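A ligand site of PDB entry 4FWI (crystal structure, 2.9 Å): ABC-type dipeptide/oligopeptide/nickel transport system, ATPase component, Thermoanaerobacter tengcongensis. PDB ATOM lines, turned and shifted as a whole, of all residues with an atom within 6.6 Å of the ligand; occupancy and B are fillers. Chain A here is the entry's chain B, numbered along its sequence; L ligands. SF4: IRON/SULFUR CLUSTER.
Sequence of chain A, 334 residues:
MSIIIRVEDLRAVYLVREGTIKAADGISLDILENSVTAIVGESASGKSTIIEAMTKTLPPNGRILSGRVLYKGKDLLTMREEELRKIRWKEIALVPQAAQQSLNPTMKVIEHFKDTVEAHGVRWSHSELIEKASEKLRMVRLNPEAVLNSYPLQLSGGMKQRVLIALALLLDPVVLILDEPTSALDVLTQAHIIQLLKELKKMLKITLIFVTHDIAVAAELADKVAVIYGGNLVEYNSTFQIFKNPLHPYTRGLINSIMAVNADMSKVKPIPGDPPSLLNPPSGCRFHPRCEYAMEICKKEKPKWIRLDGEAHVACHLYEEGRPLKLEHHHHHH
S2 of the ligand lies close to O of Tyr 293.
Residues that only touch the ligand: Pro 249 (3.5 Å), Phe 287 (3.8 Å), His 288 (3.6 Å), Ala 294 (3.99 Å), Pro 303 (3.8 Å) and Leu 318 (3.9 Å).
Of the 24 residues printed, 13 come within 4 Å of the ligand.
Along chain A the residues within 4 Å of the ligand span positions 248 to 318.
The nearest printed residue that does not touch the ligand is Met 295 (4.2 Å).
SG of Cys 291 sits close to N of Tyr 293 (3.2 Å).
The backbone NH (N) of Ala 294 sits close to the side-chain sulfur (SG) of Cys 291 (3.8 Å).
N of Cys 285 is in hydrogen-bond range of O of Cys 298.
The backbone carbonyl oxygen (O) of Cys 285 is in hydrogen-bond range of a ring nitrogen (ND1) of His 288.
The side-chain sulfur (SG) of Cys 285 sits close to the backbone NH (N) of Phe 287 (3.5 Å).
SG of Cys 298 sits close to N of Met 295 (3.1 Å).
A ring nitrogen (ND1) of His 248 lies within hydrogen-bond range of the backbone carbonyl oxygen (O) of Ala 315 (3.2 Å).
NE2 of His 317 lies within hydrogen-bond range of O of Glu 301, 2.8 Å away.
An iron atom (FE3) of the ligand is bound by the side-chain sulfur (SG) of Cys 291 (2.2 Å).
The side-chain sulfur (SG) of Cys 285 is bound to an iron atom (FE2) of the ligand (2.3 Å).
SG of Cys 298 binds FE1 of the ligand (2.3 Å).
SG of Cys 316 binds FE4 of the ligand, at 2.3 Å.
A sulfur (S1) of the ligand lies close to a ring nitrogen (NE2) of His 248 (3.2 Å).
The backbone NH (N) of His 317 sits close to a sulfur (S3) of the ligand (3.5 Å).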
ATOM      1  N   VAL A 234       3.052  12.004  18.487  1.00  0.00           N
ATOM      2  CA  VAL A 234       3.729  11.020  17.680  1.00  0.00           C
ATOM      3  C   VAL A 234       4.800  10.250  18.507  1.00  0.00           C
ATOM      4  O   VAL A 234       5.112   9.079  18.237  1.00  0.00           O
ATOM      5  CB  VAL A 234       4.325  11.757  16.453  1.00  0.00           C
ATOM      6  CG1 VAL A 234       5.806  12.035  16.623  1.00  0.00           C
ATOM      7  CG2 VAL A 234       4.076  10.996  15.202  1.00  0.00           C
ATOM      8  N   HIS A 248       9.745   7.294  16.357  1.00  0.00           N
ATOM      9  CA  HIS A 248       8.927   7.620  15.191  1.00  0.00           C
ATOM     10  C   HIS A 248       9.814   8.037  13.988  1.00  0.00           C
ATOM     11  O   HIS A 248      10.755   8.830  14.149  1.00  0.00           O
ATOM     12  CB  HIS A 248       7.858   8.698  15.483  1.00  0.00           C
ATOM     13  CG  HIS A 248       6.761   8.739  14.464  1.00  0.00           C
ATOM     14  ND1 HIS A 248       5.556   8.099  14.639  1.00  0.00           N
ATOM     15  CD2 HIS A 248       6.713   9.297  13.223  1.00  0.00           C
ATOM     16  CE1 HIS A 248       4.804   8.261  13.560  1.00  0.00           C
ATOM     17  NE2 HIS A 248       5.493   8.973  12.678  1.00  0.00           N
ATOM     18  N   PRO A 249       9.541   7.458  12.800  1.00  0.00           N
ATOM     19  CA  PRO A 249      10.198   7.873  11.553  1.00  0.00           C
ATOM     20  C   PRO A 249      10.240   9.414  11.370  1.00  0.00           C
ATOM     21  O   PRO A 249      11.240   9.959  10.901  1.00  0.00           O
ATOM     22  CB  PRO A 249       9.346   7.210  10.470  1.00  0.00           C
ATOM     23  CG  PRO A 249       8.871   5.965  11.118  1.00  0.00           C
ATOM     24  CD  PRO A 249       8.664   6.283  12.583  1.00  0.00           C
ATOM     25  N   TYR A 250       9.164  10.102  11.745  1.00  0.00           N
ATOM     26  CA  TYR A 250       9.163  11.543  11.646  1.00  0.00           C
ATOM     27  C   TYR A 250      10.242  12.154  12.531  1.00  0.00           C
ATOM     28  O   TYR A 250      11.048  12.981  12.076  1.00  0.00           O
ATOM     29  CB  TYR A 250       7.807  12.125  12.025  1.00  0.00           C
ATOM     30  CG  TYR A 250       7.847  13.626  12.142  1.00  0.00           C
ATOM     31  CD1 TYR A 250       8.282  14.418  11.076  1.00  0.00           C
ATOM     32  CD2 TYR A 250       7.503  14.265  13.329  1.00  0.00           C
ATOM     33  CE1 TYR A 250       8.352  15.796  11.188  1.00  0.00           C
ATOM     34  CE2 TYR A 250       7.577  15.635  13.453  1.00  0.00           C
ATOM     35  CZ  TYR A 250       8.000  16.408  12.379  1.00  0.00           C
ATOM     36  OH  TYR A 250       8.048  17.785  12.489  1.00  0.00           O
ATOM     37  N   CYS A 285      -2.199   6.761  10.076  1.00  0.00           N
ATOM     38  CA  CYS A 285      -1.090   7.570  10.522  1.00  0.00           C
ATOM     39  C   CYS A 285      -0.827   8.689   9.513  1.00  0.00           C
ATOM     40  O   CYS A 285      -0.352   8.454   8.391  1.00  0.00           O
ATOM     41  CB  CYS A 285       0.159   6.704  10.734  1.00  0.00           C
ATOM     42  SG  CYS A 285       1.626   7.699  10.993  1.00  0.00           S
ATOM     43  N   ARG A 286      -1.151   9.905   9.941  1.00  0.00           N
ATOM     44  CA  ARG A 286      -1.006  11.097   9.107  1.00  0.00           C
ATOM     45  C   ARG A 286       0.421  11.344   8.564  1.00  0.00           C
ATOM     46  O   ARG A 286       0.641  12.208   7.702  1.00  0.00           O
ATOM     47  CB  ARG A 286      -1.512  12.320   9.869  1.00  0.00           C
ATOM     48  CG  ARG A 286      -2.931  12.157  10.390  1.00  0.00           C
ATOM     49  CD  ARG A 286      -3.400  13.342  11.220  1.00  0.00           C
ATOM     50  NE  ARG A 286      -4.840  13.309  11.483  1.00  0.00           N
ATOM     51  CZ  ARG A 286      -5.469  14.146  12.308  1.00  0.00           C
ATOM     52  NH1 ARG A 286      -4.791  15.071  12.954  1.00  0.00           N
ATOM     53  NH2 ARG A 286      -6.784  14.051  12.478  1.00  0.00           N
ATOM     54  N   PHE A 287       1.393  10.565   9.044  1.00  0.00           N
ATOM     55  CA  PHE A 287       2.764  10.721   8.569  1.00  0.00           C
ATOM     56  C   PHE A 287       3.037   9.802   7.371  1.00  0.00           C
ATOM     57  O   PHE A 287       4.028   9.996   6.668  1.00  0.00           O
ATOM     58  CB  PHE A 287       3.818  10.568   9.690  1.00  0.00           C
ATOM     59  CG  PHE A 287       5.234  10.744   9.204  1.00  0.00           C
ATOM     60  CD1 PHE A 287       5.604  11.901   8.496  1.00  0.00           C
ATOM     61  CD2 PHE A 287       6.199   9.760   9.423  1.00  0.00           C
ATOM     62  CE1 PHE A 287       6.912  12.076   8.019  1.00  0.00           C
ATOM     63  CE2 PHE A 287       7.495   9.915   8.938  1.00  0.00           C
ATOM     64  CZ  PHE A 287       7.860  11.067   8.238  1.00  0.00           C
ATOM     65  N   HIS A 288       2.137   8.854   7.124  1.00  0.00           N
ATOM     66  CA  HIS A 288       2.387   7.848   6.087  1.00  0.00           C
ATOM     67  C   HIS A 288       2.785   8.421   4.701  1.00  0.00           C
ATOM     68  O   HIS A 288       3.758   7.969   4.097  1.00  0.00           O
ATOM     69  CB  HIS A 288       1.281   6.763   6.022  1.00  0.00           C
ATOM     70  CG  HIS A 288       0.014   7.181   5.328  1.00  0.00           C
ATOM     71  ND1 HIS A 288      -1.184   7.346   5.992  1.00  0.00           N
ATOM     72  CD2 HIS A 288      -0.261   7.401   4.017  1.00  0.00           C
ATOM     73  CE1 HIS A 288      -2.131   7.680   5.127  1.00  0.00           C
ATOM     74  NE2 HIS A 288      -1.596   7.720   3.923  1.00  0.00           N
ATOM     75  N   PRO A 289       2.079   9.453   4.221  1.00  0.00           N
ATOM     76  CA  PRO A 289       2.418  10.017   2.901  1.00  0.00           C
ATOM     77  C   PRO A 289       3.860  10.524   2.784  1.00  0.00           C
ATOM     78  O   PRO A 289       4.325  10.836   1.684  1.00  0.00           O
ATOM     79  CB  PRO A 289       1.451  11.194   2.751  1.00  0.00           C
ATOM     80  CG  PRO A 289       0.304  10.859   3.669  1.00  0.00           C
ATOM     81  CD  PRO A 289       0.893  10.115   4.821  1.00  0.00           C
ATOM     82  N   CYS A 291       6.303   9.164   5.165  1.00  0.00           N
ATOM     83  CA  CYS A 291       7.077   8.124   5.822  1.00  0.00           C
ATOM     84  C   CYS A 291       7.676   7.081   4.870  1.00  0.00           C
ATOM     85  O   CYS A 291       6.979   6.492   4.035  1.00  0.00           O
ATOM     86  CB  CYS A 291       6.229   7.421   6.863  1.00  0.00           C
ATOM     87  SG  CYS A 291       7.266   6.245   7.661  1.00  0.00           S
ATOM     88  N   GLU A 292       8.975   6.820   5.018  1.00  0.00           N
ATOM     89  CA  GLU A 292       9.630   5.880   4.116  1.00  0.00           C
ATOM     90  C   GLU A 292       9.369   4.426   4.497  1.00  0.00           C
ATOM     91  O   GLU A 292       9.637   3.523   3.717  1.00  0.00           O
ATOM     92  CB  GLU A 292      11.123   6.147   4.013  1.00  0.00           C
ATOM     93  CG  GLU A 292      11.923   5.772   5.259  1.00  0.00           C
ATOM     94  CD  GLU A 292      13.432   5.667   4.978  1.00  0.00           C
ATOM     95  OE1 GLU A 292      14.217   6.363   5.668  1.00  0.00           O
ATOM     96  OE2 GLU A 292      13.827   4.885   4.074  1.00  0.00           O
ATOM     97  N   TYR A 293       8.813   4.217   5.686  1.00  0.00           N
ATOM     98  CA  TYR A 293       8.470   2.872   6.165  1.00  0.00           C
ATOM     99  C   TYR A 293       6.969   2.627   6.114  1.00  0.00           C
ATOM    100  O   TYR A 293       6.471   1.703   6.751  1.00  0.00           O
ATOM    101  CB  TYR A 293       8.973   2.695   7.588  1.00  0.00           C
ATOM    102  CG  TYR A 293      10.448   2.933   7.687  1.00  0.00           C
ATOM    103  CD1 TYR A 293      11.348   2.048   7.093  1.00  0.00           C
ATOM    104  CD2 TYR A 293      10.957   4.049   8.345  1.00  0.00           C
ATOM    105  CE1 TYR A 293      12.718   2.261   7.161  1.00  0.00           C
ATOM    106  CE2 TYR A 293      12.336   4.269   8.422  1.00  0.00           C
ATOM    107  CZ  TYR A 293      13.210   3.361   7.824  1.00  0.00           C
ATOM    108  OH  TYR A 293      14.569   3.538   7.874  1.00  0.00           O
ATOM    109  N   ALA A 294       6.273   3.460   5.345  1.00  0.00           N
ATOM    110  CA  ALA A 294       4.822   3.397   5.213  1.00  0.00           C
ATOM    111  C   ALA A 294       4.306   2.028   4.741  1.00  0.00           C
ATOM    112  O   ALA A 294       4.914   1.373   3.884  1.00  0.00           O
ATOM    113  CB  ALA A 294       4.354   4.489   4.274  1.00  0.00           C
ATOM    114  N   MET A 295       3.179   1.600   5.311  1.00  0.00           N
ATOM    115  CA  MET A 295       2.592   0.300   4.987  1.00  0.00           C
ATOM    116  C   MET A 295       1.082   0.425   4.787  1.00  0.00           C
ATOM    117  O   MET A 295       0.535   1.522   4.879  1.00  0.00           O
ATOM    118  CB  MET A 295       2.899  -0.718   6.072  1.00  0.00           C
ATOM    119  CG  MET A 295       4.386  -1.110   6.150  1.00  0.00           C
ATOM    120  SD  MET A 295       4.869  -1.880   7.720  1.00  0.00           S
ATOM    121  CE  MET A 295       4.708  -0.490   8.849  1.00  0.00           C
ATOM    122  N   ILE A 297      -1.400  -0.944   6.671  1.00  0.00           N
ATOM    123  CA  ILE A 297      -2.000  -0.708   7.971  1.00  0.00           C
ATOM    124  C   ILE A 297      -1.802   0.742   8.406  1.00  0.00           C
ATOM    125  O   ILE A 297      -2.593   1.277   9.186  1.00  0.00           O
ATOM    126  CB  ILE A 297      -1.374  -1.659   9.025  1.00  0.00           C
ATOM    127  CG1 ILE A 297      -2.112  -1.575  10.366  1.00  0.00           C
ATOM    128  CG2 ILE A 297       0.134  -1.368   9.194  1.00  0.00           C
ATOM    129  CD1 ILE A 297      -1.580  -2.563  11.429  1.00  0.00           C
ATOM    130  N   CYS A 298      -0.752   1.382   7.883  1.00  0.00           N
ATOM    131  CA  CYS A 298      -0.439   2.779   8.224  1.00  0.00           C
ATOM    132  C   CYS A 298      -1.470   3.739   7.630  1.00  0.00           C
ATOM    133  O   CYS A 298      -1.636   4.863   8.131  1.00  0.00           O
ATOM    134  CB  CYS A 298       0.958   3.156   7.733  1.00  0.00           C
ATOM    135  SG  CYS A 298       2.269   2.026   8.197  1.00  0.00           S
ATOM    136  N   LYS A 299      -2.129   3.331   6.556  1.00  0.00           N
ATOM    137  CA  LYS A 299      -3.174   4.166   5.954  1.00  0.00           C
ATOM    138  C   LYS A 299      -4.561   3.725   6.397  1.00  0.00           C
ATOM    139  O   LYS A 299      -5.489   4.528   6.425  1.00  0.00           O
ATOM    140  CB  LYS A 299      -3.059   4.225   4.414  1.00  0.00           C
ATOM    141  CG  LYS A 299      -2.585   2.939   3.753  1.00  0.00           C
ATOM    142  CD  LYS A 299      -2.429   3.156   2.249  1.00  0.00           C
ATOM    143  CE  LYS A 299      -1.487   4.309   1.948  1.00  0.00           C
ATOM    144  NZ  LYS A 299      -0.076   4.053   2.392  1.00  0.00           N
ATOM    145  N   GLU A 301      -5.153   2.485   9.446  1.00  0.00           N
ATOM    146  CA  GLU A 301      -5.308   2.500  10.897  1.00  0.00           C
ATOM    147  C   GLU A 301      -4.339   3.448  11.656  1.00  0.00           C
ATOM    148  O   GLU A 301      -3.144   3.502  11.366  1.00  0.00           O
ATOM    149  CB  GLU A 301      -5.265   1.060  11.408  1.00  0.00           C
ATOM    150  CG  GLU A 301      -5.669   0.865  12.844  1.00  0.00           C
ATOM    151  CD  GLU A 301      -5.279  -0.496  13.364  1.00  0.00           C
ATOM    152  OE1 GLU A 301      -5.724  -1.511  12.760  1.00  0.00           O
ATOM    153  OE2 GLU A 301      -4.511  -0.563  14.365  1.00  0.00           O
ATOM    154  N   PRO A 303      -1.878   4.401  14.301  1.00  0.00           N
ATOM    155  CA  PRO A 303      -1.048   3.592  15.201  1.00  0.00           C
ATOM    156  C   PRO A 303      -1.366   3.936  16.649  1.00  0.00           C
ATOM    157  O   PRO A 303      -1.568   5.107  16.951  1.00  0.00           O
ATOM    158  CB  PRO A 303       0.395   3.965  14.819  1.00  0.00           C
ATOM    159  CG  PRO A 303       0.277   5.243  14.044  1.00  0.00           C
ATOM    160  CD  PRO A 303      -1.083   5.282  13.423  1.00  0.00           C
ATOM    161  N   ALA A 315       3.693   6.208  18.727  1.00  0.00           N
ATOM    162  CA  ALA A 315       2.460   5.833  18.071  1.00  0.00           C
ATOM    163  C   ALA A 315       2.912   5.538  16.675  1.00  0.00           C
ATOM    164  O   ALA A 315       3.134   6.465  15.883  1.00  0.00           O
ATOM    165  CB  ALA A 315       1.477   6.966  18.088  1.00  0.00           C
ATOM    166  N   CYS A 316       3.058   4.251  16.383  1.00  0.00           N
ATOM    167  CA  CYS A 316       3.729   3.769  15.189  1.00  0.00           C
ATOM    168  C   CYS A 316       3.539   2.289  15.040  1.00  0.00           C
ATOM    169  O   CYS A 316       3.748   1.551  15.997  1.00  0.00           O
ATOM    170  CB  CYS A 316       5.220   4.028  15.312  1.00  0.00           C
ATOM    171  SG  CYS A 316       6.080   3.656  13.824  1.00  0.00           S
ATOM    172  N   HIS A 317       3.150   1.852  13.853  1.00  0.00           N
ATOM    173  CA  HIS A 317       2.913   0.429  13.641  1.00  0.00           C
ATOM    174  C   HIS A 317       4.183  -0.422  13.754  1.00  0.00           C
ATOM    175  O   HIS A 317       4.118  -1.615  14.094  1.00  0.00           O
ATOM    176  CB  HIS A 317       2.223   0.199  12.307  1.00  0.00           C
ATOM    177  CG  HIS A 317       0.819   0.717  12.283  1.00  0.00           C
ATOM    178  ND1 HIS A 317      -0.104   0.387  13.259  1.00  0.00           N
ATOM    179  CD2 HIS A 317       0.184   1.536  11.410  1.00  0.00           C
ATOM    180  CE1 HIS A 317      -1.258   0.964  12.975  1.00  0.00           C
ATOM    181  NE2 HIS A 317      -1.109   1.667  11.865  1.00  0.00           N
ATOM    182  N   LEU A 318       5.336   0.189  13.485  1.00  0.00           N
ATOM    183  CA  LEU A 318       6.613  -0.512  13.564  1.00  0.00           C
ATOM    184  C   LEU A 318       6.902  -1.092  14.950  1.00  0.00           C
ATOM    185  O   LEU A 318       7.727  -1.998  15.099  1.00  0.00           O
ATOM    186  CB  LEU A 318       7.758   0.411  13.165  1.00  0.00           C
ATOM    187  CG  LEU A 318       7.814   0.857  11.715  1.00  0.00           C
ATOM    188  CD1 LEU A 318       9.183   1.435  11.391  1.00  0.00           C
ATOM    189  CD2 LEU A 318       7.506  -0.321  10.836  1.00  0.00           C
ATOM    190  N   TYR A 319       6.229  -0.563  15.968  1.00  0.00           N
ATOM    191  CA  TYR A 319       6.544  -0.930  17.334  1.00  0.00           C
ATOM    192  C   TYR A 319       5.393  -1.671  18.052  1.00  0.00           C
ATOM    193  O   TYR A 319       4.316  -1.896  17.475  1.00  0.00           O
ATOM    194  CB  TYR A 319       7.000   0.308  18.131  1.00  0.00           C
ATOM    195  CG  TYR A 319       8.155   1.059  17.476  1.00  0.00           C
ATOM    196  CD1 TYR A 319       9.472   0.731  17.757  1.00  0.00           C
ATOM    197  CD2 TYR A 319       7.920   2.082  16.566  1.00  0.00           C
ATOM    198  CE1 TYR A 319      10.537   1.398  17.151  1.00  0.00           C
ATOM    199  CE2 TYR A 319       8.980   2.764  15.953  1.00  0.00           C
ATOM    200  CZ  TYR A 319      10.293   2.411  16.255  1.00  0.00           C
ATOM    201  OH  TYR A 319      11.351   3.082  15.662  1.00  0.00           O
HETATM  202 FE1  SF4 L   1       3.334   3.510   9.574  1.00  0.00          FE
HETATM  203 FE2  SF4 L   1       3.272   6.293  10.365  1.00  0.00          FE
HETATM  204 FE3  SF4 L   1       5.677   5.391   8.958  1.00  0.00          FE
HETATM  205 FE4  SF4 L   1       5.175   4.443  11.806  1.00  0.00          FE
HETATM  206  S1  SF4 L   1       5.387   6.382  10.848  1.00  0.00           S
HETATM  207  S2  SF4 L   1       5.491   3.445   9.929  1.00  0.00           S
HETATM  208  S3  SF4 L   1       2.994   4.464  11.502  1.00  0.00           S
HETATM  209  S4  SF4 L   1       3.579   5.375   8.452  1.00  0.00           S
